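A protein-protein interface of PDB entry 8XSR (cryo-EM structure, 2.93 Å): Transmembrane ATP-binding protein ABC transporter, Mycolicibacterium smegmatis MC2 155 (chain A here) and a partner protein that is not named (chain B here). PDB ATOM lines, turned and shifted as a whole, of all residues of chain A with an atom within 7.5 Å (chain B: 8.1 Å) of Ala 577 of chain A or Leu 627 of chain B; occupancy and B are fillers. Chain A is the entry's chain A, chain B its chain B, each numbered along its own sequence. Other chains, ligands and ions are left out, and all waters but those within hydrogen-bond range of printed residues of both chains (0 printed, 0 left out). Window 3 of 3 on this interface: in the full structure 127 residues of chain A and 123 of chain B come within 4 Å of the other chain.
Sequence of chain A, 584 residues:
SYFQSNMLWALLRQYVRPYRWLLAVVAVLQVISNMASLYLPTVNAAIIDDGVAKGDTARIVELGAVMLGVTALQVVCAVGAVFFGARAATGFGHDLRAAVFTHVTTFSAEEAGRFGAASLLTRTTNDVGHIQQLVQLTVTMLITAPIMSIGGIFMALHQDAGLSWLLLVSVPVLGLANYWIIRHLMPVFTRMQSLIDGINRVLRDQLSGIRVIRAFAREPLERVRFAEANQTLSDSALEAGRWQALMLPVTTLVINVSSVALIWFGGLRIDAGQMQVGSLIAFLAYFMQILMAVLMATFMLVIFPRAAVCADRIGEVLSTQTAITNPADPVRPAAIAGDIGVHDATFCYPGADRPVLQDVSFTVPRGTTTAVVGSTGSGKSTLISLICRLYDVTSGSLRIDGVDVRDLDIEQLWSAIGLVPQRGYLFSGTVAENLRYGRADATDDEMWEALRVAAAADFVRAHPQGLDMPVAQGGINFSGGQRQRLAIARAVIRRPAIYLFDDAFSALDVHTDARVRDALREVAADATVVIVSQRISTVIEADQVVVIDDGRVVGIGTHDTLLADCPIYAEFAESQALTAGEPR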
ATOM      1  N   VAL A 510     -11.241  -2.495   1.094  1.00  0.00           N
ATOM      2  CA  VAL A 510     -11.031  -2.465  -0.350  1.00  0.00           C
ATOM      3  C   VAL A 510     -11.652  -3.685  -1.016  1.00  0.00           C
ATOM      4  O   VAL A 510     -12.162  -3.601  -2.141  1.00  0.00           O
ATOM      5  CB  VAL A 510      -9.523  -2.352  -0.655  1.00  0.00           C
ATOM      6  CG1 VAL A 510      -9.270  -2.371  -2.154  1.00  0.00           C
ATOM      7  CG2 VAL A 510      -8.956  -1.089  -0.029  1.00  0.00           C
ATOM      8  N   PHE A 572      -2.139  13.157  -3.746  1.00  0.00           N
ATOM      9  CA  PHE A 572      -3.289  12.561  -3.088  1.00  0.00           C
ATOM     10  C   PHE A 572      -3.182  11.046  -3.058  1.00  0.00           C
ATOM     11  O   PHE A 572      -3.526  10.420  -2.052  1.00  0.00           O
ATOM     12  CB  PHE A 572      -4.554  12.980  -3.834  1.00  0.00           C
ATOM     13  CG  PHE A 572      -5.812  12.764  -3.071  1.00  0.00           C
ATOM     14  CD1 PHE A 572      -6.286  13.738  -2.212  1.00  0.00           C
ATOM     15  CD2 PHE A 572      -6.510  11.587  -3.187  1.00  0.00           C
ATOM     16  CE1 PHE A 572      -7.444  13.547  -1.515  1.00  0.00           C
ATOM     17  CE2 PHE A 572      -7.659  11.387  -2.488  1.00  0.00           C
ATOM     18  CZ  PHE A 572      -8.132  12.367  -1.643  1.00  0.00           C
ATOM     19  N   ALA A 573      -2.728  10.451  -4.160  1.00  0.00           N
ATOM     20  CA  ALA A 573      -2.526   9.010  -4.234  1.00  0.00           C
ATOM     21  C   ALA A 573      -1.265   8.560  -3.516  1.00  0.00           C
ATOM     22  O   ALA A 573      -1.172   7.390  -3.133  1.00  0.00           O
ATOM     23  CB  ALA A 573      -2.474   8.559  -5.696  1.00  0.00           C
ATOM     24  N   GLU A 574      -0.297   9.453  -3.328  1.00  0.00           N
ATOM     25  CA  GLU A 574       0.912   9.136  -2.585  1.00  0.00           C
ATOM     26  C   GLU A 574       0.679   9.082  -1.082  1.00  0.00           C
ATOM     27  O   GLU A 574       1.393   8.353  -0.386  1.00  0.00           O
ATOM     28  CB  GLU A 574       2.004  10.161  -2.909  1.00  0.00           C
ATOM     29  CG  GLU A 574       3.356   9.860  -2.290  1.00  0.00           C
ATOM     30  CD  GLU A 574       4.422  10.850  -2.707  1.00  0.00           C
ATOM     31  OE1 GLU A 574       4.101  11.783  -3.473  1.00  0.00           O
ATOM     32  OE2 GLU A 574       5.582  10.696  -2.269  1.00  0.00           O
ATOM     33  N   SER A 575      -0.307   9.812  -0.568  1.00  0.00           N
ATOM     34  CA  SER A 575      -0.683   9.740   0.835  1.00  0.00           C
ATOM     35  C   SER A 575      -1.424   8.455   1.169  1.00  0.00           C
ATOM     36  O   SER A 575      -1.846   8.274   2.314  1.00  0.00           O
ATOM     37  CB  SER A 575      -1.544  10.942   1.217  1.00  0.00           C
ATOM     38  OG  SER A 575      -2.802  10.883   0.572  1.00  0.00           O
ATOM     39  N   GLN A 576      -1.600   7.566   0.192  1.00  0.00           N
ATOM     40  CA  GLN A 576      -2.230   6.277   0.417  1.00  0.00           C
ATOM     41  C   GLN A 576      -1.354   5.112  -0.013  1.00  0.00           C
ATOM     42  O   GLN A 576      -1.801   3.963   0.068  1.00  0.00           O
ATOM     43  CB  GLN A 576      -3.576   6.202  -0.316  1.00  0.00           C
ATOM     44  CG  GLN A 576      -4.600   7.178   0.212  1.00  0.00           C
ATOM     45  CD  GLN A 576      -5.917   7.088  -0.515  1.00  0.00           C
ATOM     46  OE1 GLN A 576      -6.067   6.306  -1.451  1.00  0.00           O
ATOM     47  NE2 GLN A 576      -6.881   7.893  -0.096  1.00  0.00           N
ATOM     48  N   ALA A 577      -0.133   5.379  -0.479  1.00  0.00           N
ATOM     49  CA  ALA A 577       0.851   4.357  -0.829  1.00  0.00           C
ATOM     50  C   ALA A 577       0.397   3.479  -1.989  1.00  0.00           C
ATOM     51  O   ALA A 577       0.446   2.250  -1.900  1.00  0.00           O
ATOM     52  CB  ALA A 577       1.213   3.491   0.382  1.00  0.00           C
ATOM     53  N   LEU A 578      -0.050   4.090  -3.081  1.00  0.00           N
ATOM     54  CA  LEU A 578      -0.337   3.344  -4.303  1.00  0.00           C
ATOM     55  C   LEU A 578       0.892   3.303  -5.204  1.00  0.00           C
ATOM     56  O   LEU A 578       0.895   2.637  -6.238  1.00  0.00           O
ATOM     57  CB  LEU A 578      -1.521   3.953  -5.061  1.00  0.00           C
ATOM     58  CG  LEU A 578      -2.932   3.560  -4.616  1.00  0.00           C
ATOM     59  CD1 LEU A 578      -3.300   4.203  -3.295  1.00  0.00           C
ATOM     60  CD2 LEU A 578      -3.941   3.927  -5.688  1.00  0.00           C
ATOM     61  N   THR B 560      -6.987  12.133   3.745  1.00  0.00           N
ATOM     62  CA  THR B 560      -5.727  11.474   4.060  1.00  0.00           C
ATOM     63  C   THR B 560      -4.571  12.236   3.431  1.00  0.00           C
ATOM     64  O   THR B 560      -3.405  11.890   3.633  1.00  0.00           O
ATOM     65  CB  THR B 560      -5.733  10.029   3.578  1.00  0.00           C
ATOM     66  OG1 THR B 560      -4.575   9.356   4.082  1.00  0.00           O
ATOM     67  CG2 THR B 560      -5.706   9.995   2.073  1.00  0.00           C
ATOM     68  N   LEU B 564      -1.525  14.064   5.654  1.00  0.00           N
ATOM     69  CA  LEU B 564      -0.114  13.950   5.314  1.00  0.00           C
ATOM     70  C   LEU B 564       0.583  15.299   5.248  1.00  0.00           C
ATOM     71  O   LEU B 564       1.801  15.352   5.426  1.00  0.00           O
ATOM     72  CB  LEU B 564       0.057  13.224   3.977  1.00  0.00           C
ATOM     73  CG  LEU B 564       1.495  12.894   3.564  1.00  0.00           C
ATOM     74  CD1 LEU B 564       2.104  11.889   4.523  1.00  0.00           C
ATOM     75  CD2 LEU B 564       1.572  12.394   2.136  1.00  0.00           C
ATOM     76  N   LEU B 586      -2.139   4.122   8.240  1.00  0.00           N
ATOM     77  CA  LEU B 586      -0.684   4.053   8.373  1.00  0.00           C
ATOM     78  C   LEU B 586       0.036   4.217   7.046  1.00  0.00           C
ATOM     79  O   LEU B 586       1.205   3.845   6.914  1.00  0.00           O
ATOM     80  CB  LEU B 586      -0.295   2.747   9.060  1.00  0.00           C
ATOM     81  CG  LEU B 586      -0.747   1.408   8.479  1.00  0.00           C
ATOM     82  CD1 LEU B 586       0.208   0.897   7.423  1.00  0.00           C
ATOM     83  CD2 LEU B 586      -0.891   0.396   9.593  1.00  0.00           C
ATOM     84  N   SER B 587      -0.629   4.787   6.045  1.00  0.00           N
ATOM     85  CA  SER B 587       0.035   5.208   4.823  1.00  0.00           C
ATOM     86  C   SER B 587       0.590   6.617   4.939  1.00  0.00           C
ATOM     87  O   SER B 587       1.461   6.995   4.148  1.00  0.00           O
ATOM     88  CB  SER B 587      -0.929   5.123   3.634  1.00  0.00           C
ATOM     89  OG  SER B 587      -1.992   6.049   3.771  1.00  0.00           O
ATOM     90  N   THR B 588       0.106   7.405   5.898  1.00  0.00           N
ATOM     91  CA  THR B 588       0.718   8.674   6.253  1.00  0.00           C
ATOM     92  C   THR B 588       1.818   8.513   7.291  1.00  0.00           C
ATOM     93  O   THR B 588       2.537   9.478   7.572  1.00  0.00           O
ATOM     94  CB  THR B 588      -0.341   9.644   6.789  1.00  0.00           C
ATOM     95  OG1 THR B 588      -0.878   9.135   8.013  1.00  0.00           O
ATOM     96  CG2 THR B 588      -1.473   9.787   5.792  1.00  0.00           C
ATOM     97  N   ARG B 590       4.279   6.023   7.026  1.00  0.00           N
ATOM     98  CA  ARG B 590       5.527   5.681   6.362  1.00  0.00           C
ATOM     99  C   ARG B 590       6.385   6.929   6.196  1.00  0.00           C
ATOM    100  O   ARG B 590       5.868   8.042   6.059  1.00  0.00           O
ATOM    101  CB  ARG B 590       5.256   5.026   5.008  1.00  0.00           C
ATOM    102  CG  ARG B 590       4.590   5.919   3.986  1.00  0.00           C
ATOM    103  CD  ARG B 590       4.372   5.162   2.689  1.00  0.00           C
ATOM    104  NE  ARG B 590       3.658   5.958   1.699  1.00  0.00           N
ATOM    105  CZ  ARG B 590       4.246   6.781   0.840  1.00  0.00           C
ATOM    106  NH1 ARG B 590       3.517   7.466  -0.028  1.00  0.00           N
ATOM    107  NH2 ARG B 590       5.564   6.921   0.850  1.00  0.00           N
ATOM    108  N   HIS B 609      10.487   2.687   8.549  1.00  0.00           N
ATOM    109  CA  HIS B 609       9.585   2.059   7.590  1.00  0.00           C
ATOM    110  C   HIS B 609      10.246   0.896   6.864  1.00  0.00           C
ATOM    111  O   HIS B 609       9.665  -0.189   6.777  1.00  0.00           O
ATOM    112  CB  HIS B 609       9.074   3.084   6.581  1.00  0.00           C
ATOM    113  CG  HIS B 609       8.186   2.496   5.530  1.00  0.00           C
ATOM    114  ND1 HIS B 609       6.912   2.048   5.798  1.00  0.00           N
ATOM    115  CD2 HIS B 609       8.390   2.283   4.209  1.00  0.00           C
ATOM    116  CE1 HIS B 609       6.369   1.581   4.688  1.00  0.00           C
ATOM    117  NE2 HIS B 609       7.245   1.714   3.708  1.00  0.00           N
ATOM    118  N   MET B 622       0.200  -5.470   7.876  1.00  0.00           N
ATOM    119  CA  MET B 622      -0.732  -4.358   7.997  1.00  0.00           C
ATOM    120  C   MET B 622      -0.627  -3.365   6.853  1.00  0.00           C
ATOM    121  O   MET B 622      -1.617  -2.690   6.553  1.00  0.00           O
ATOM    122  CB  MET B 622      -0.526  -3.610   9.322  1.00  0.00           C
ATOM    123  CG  MET B 622      -0.979  -4.373  10.553  1.00  0.00           C
ATOM    124  SD  MET B 622      -0.640  -3.495  12.090  1.00  0.00           S
ATOM    125  CE  MET B 622      -1.855  -2.187  12.010  1.00  0.00           C
ATOM    126  N   THR B 623       0.537  -3.258   6.213  1.00  0.00           N
ATOM    127  CA  THR B 623       0.700  -2.439   5.019  1.00  0.00           C
ATOM    128  C   THR B 623       0.176  -3.147   3.773  1.00  0.00           C
ATOM    129  O   THR B 623       0.357  -2.661   2.654  1.00  0.00           O
ATOM    130  CB  THR B 623       2.163  -2.050   4.816  1.00  0.00           C
ATOM    131  OG1 THR B 623       2.961  -3.233   4.689  1.00  0.00           O
ATOM    132  CG2 THR B 623       2.670  -1.220   5.975  1.00  0.00           C
ATOM    133  N   ARG B 624      -0.470  -4.299   3.950  1.00  0.00           N
ATOM    134  CA  ARG B 624      -0.966  -5.074   2.819  1.00  0.00           C
ATOM    135  C   ARG B 624      -2.383  -5.564   3.094  1.00  0.00           C
ATOM    136  O   ARG B 624      -2.747  -6.692   2.744  1.00  0.00           O
ATOM    137  CB  ARG B 624      -0.039  -6.249   2.500  1.00  0.00           C
ATOM    138  CG  ARG B 624       1.325  -5.825   1.984  1.00  0.00           C
ATOM    139  CD  ARG B 624       2.199  -7.020   1.653  1.00  0.00           C
ATOM    140  NE  ARG B 624       3.538  -6.608   1.243  1.00  0.00           N
ATOM    141  CZ  ARG B 624       3.882  -6.323  -0.008  1.00  0.00           C
ATOM    142  NH1 ARG B 624       2.983  -6.404  -0.980  1.00  0.00           N
ATOM    143  NH2 ARG B 624       5.124  -5.955  -0.288  1.00  0.00           N
ATOM    144  N   VAL B 625      -3.197  -4.720   3.727  1.00  0.00           N
ATOM    145  CA  VAL B 625      -4.610  -5.015   3.934  1.00  0.00           C
ATOM    146  C   VAL B 625      -5.414  -4.007   3.128  1.00  0.00           C
ATOM    147  O   VAL B 625      -6.506  -4.310   2.635  1.00  0.00           O
ATOM    148  CB  VAL B 625      -4.980  -4.975   5.428  1.00  0.00           C
ATOM    149  CG1 VAL B 625      -6.475  -5.187   5.624  1.00  0.00           C
ATOM    150  CG2 VAL B 625      -4.196  -6.023   6.192  1.00  0.00           C
ATOM    151  N   HIS B 626      -4.863  -2.807   2.967  1.00  0.00           N
ATOM    152  CA  HIS B 626      -5.413  -1.806   2.067  1.00  0.00           C
ATOM    153  C   HIS B 626      -4.918  -1.984   0.639  1.00  0.00           C
ATOM    154  O   HIS B 626      -5.377  -1.271  -0.259  1.00  0.00           O
ATOM    155  CB  HIS B 626      -5.071  -0.399   2.566  1.00  0.00           C
ATOM    156  CG  HIS B 626      -5.722  -0.044   3.867  1.00  0.00           C
ATOM    157  ND1 HIS B 626      -7.056   0.289   3.964  1.00  0.00           N
ATOM    158  CD2 HIS B 626      -5.224   0.028   5.123  1.00  0.00           C
ATOM    159  CE1 HIS B 626      -7.351   0.553   5.224  1.00  0.00           C
ATOM    160  NE2 HIS B 626      -6.257   0.401   5.949  1.00  0.00           N
ATOM    161  N   LEU B 627      -3.995  -2.913   0.417  1.00  0.00           N
ATOM    162  CA  LEU B 627      -3.464  -3.223  -0.904  1.00  0.00           C
ATOM    163  C   LEU B 627      -3.568  -4.732  -1.117  1.00  0.00           C
ATOM    164  O   LEU B 627      -2.646  -5.395  -1.588  1.00  0.00           O
ATOM    165  CB  LEU B 627      -2.027  -2.726  -1.049  1.00  0.00           C
ATOM    166  CG  LEU B 627      -1.779  -1.241  -1.339  1.00  0.00           C
ATOM    167  CD1 LEU B 627      -2.011  -0.375  -0.108  1.00  0.00           C
ATOM    168  CD2 LEU B 627      -0.374  -1.036  -1.885  1.00  0.00           C
ATOM    169  N   GLY B 628      -4.716  -5.297  -0.758  1.00  0.00           N
ATOM    170  CA  GLY B 628      -4.940  -6.724  -0.896  1.00  0.00           C
ATOM    171  C   GLY B 628      -4.267  -7.544   0.186  1.00  0.00           C
ATOM    172  O   GLY B 628      -4.894  -7.921   1.174  1.00  0.00           O
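O of Thr 560 of chain B sits close to OG of Ser 575 of chain A, 3.3 Å away.
The backbone carbonyl oxygen of Ser 575 of chain A is in hydrogen-bond range of the side-chain hydroxyl of Ser 587 of chain B, at 2.7 Å.
NH1 of Arg 590 of chain B sits close to O of Glu 574 of chain A.
The guanidinium group of Arg 590 of chain B lies close to the backbone carbonyl oxygen of Ser 587 of chain B, 3.4 Å away.
The backbone carbonyl oxygen (O) of Phe 572 of chain A sits at hydrogen-bond distance from the side-chain hydroxyl (OG) of Ser 575 of chain A (2.8 Å).
Of chain B, only Arg 590 and Leu 627 come within 4 Å of Ala 577 of chain A.
Of chain A, only Ala 577 (3.4 Å) comes within 4 Å of Leu 627 of chain B.
Of the printed residues of chain B, Gln 576 of chain A touches Thr 560 (3.2 Å) and Ser 587 (3.4 Å).
Of the printed residues of chain B, Ser 575 of chain A touches Thr 560 (3.2 Å), Leu 564 (3.6 Å), Ser 587 (2.7 Å) and Thr 588 (3.8 Å).
Leu 578 of chain A touches none of the printed residues of chain B.
Hydrophobic or aromatic side chains of chain A that line the printed part of chain B: Val 510 and Ala 577.
Among the printed residues, no Asp or Glu carboxylate lies within 4 Å of a Lys or Arg side-chain nitrogen of the other chain.
Val 510 of chain A touches His 626 of chain B.
CD2 of Leu 564 of chain B touches CB of Ser 575 of chain A, at 3.6 Å.
Thr 588 of chain B touches Ser 575 of chain A.
Gln 576 of chain A touches Thr 560 of chain B.
Gln 576 of chain A touches Ser 587 of chain B.
Arg 590 of chain B touches Ala 577 of chain A.
Ala 577 of chain A touches Leu 627 of chain B.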
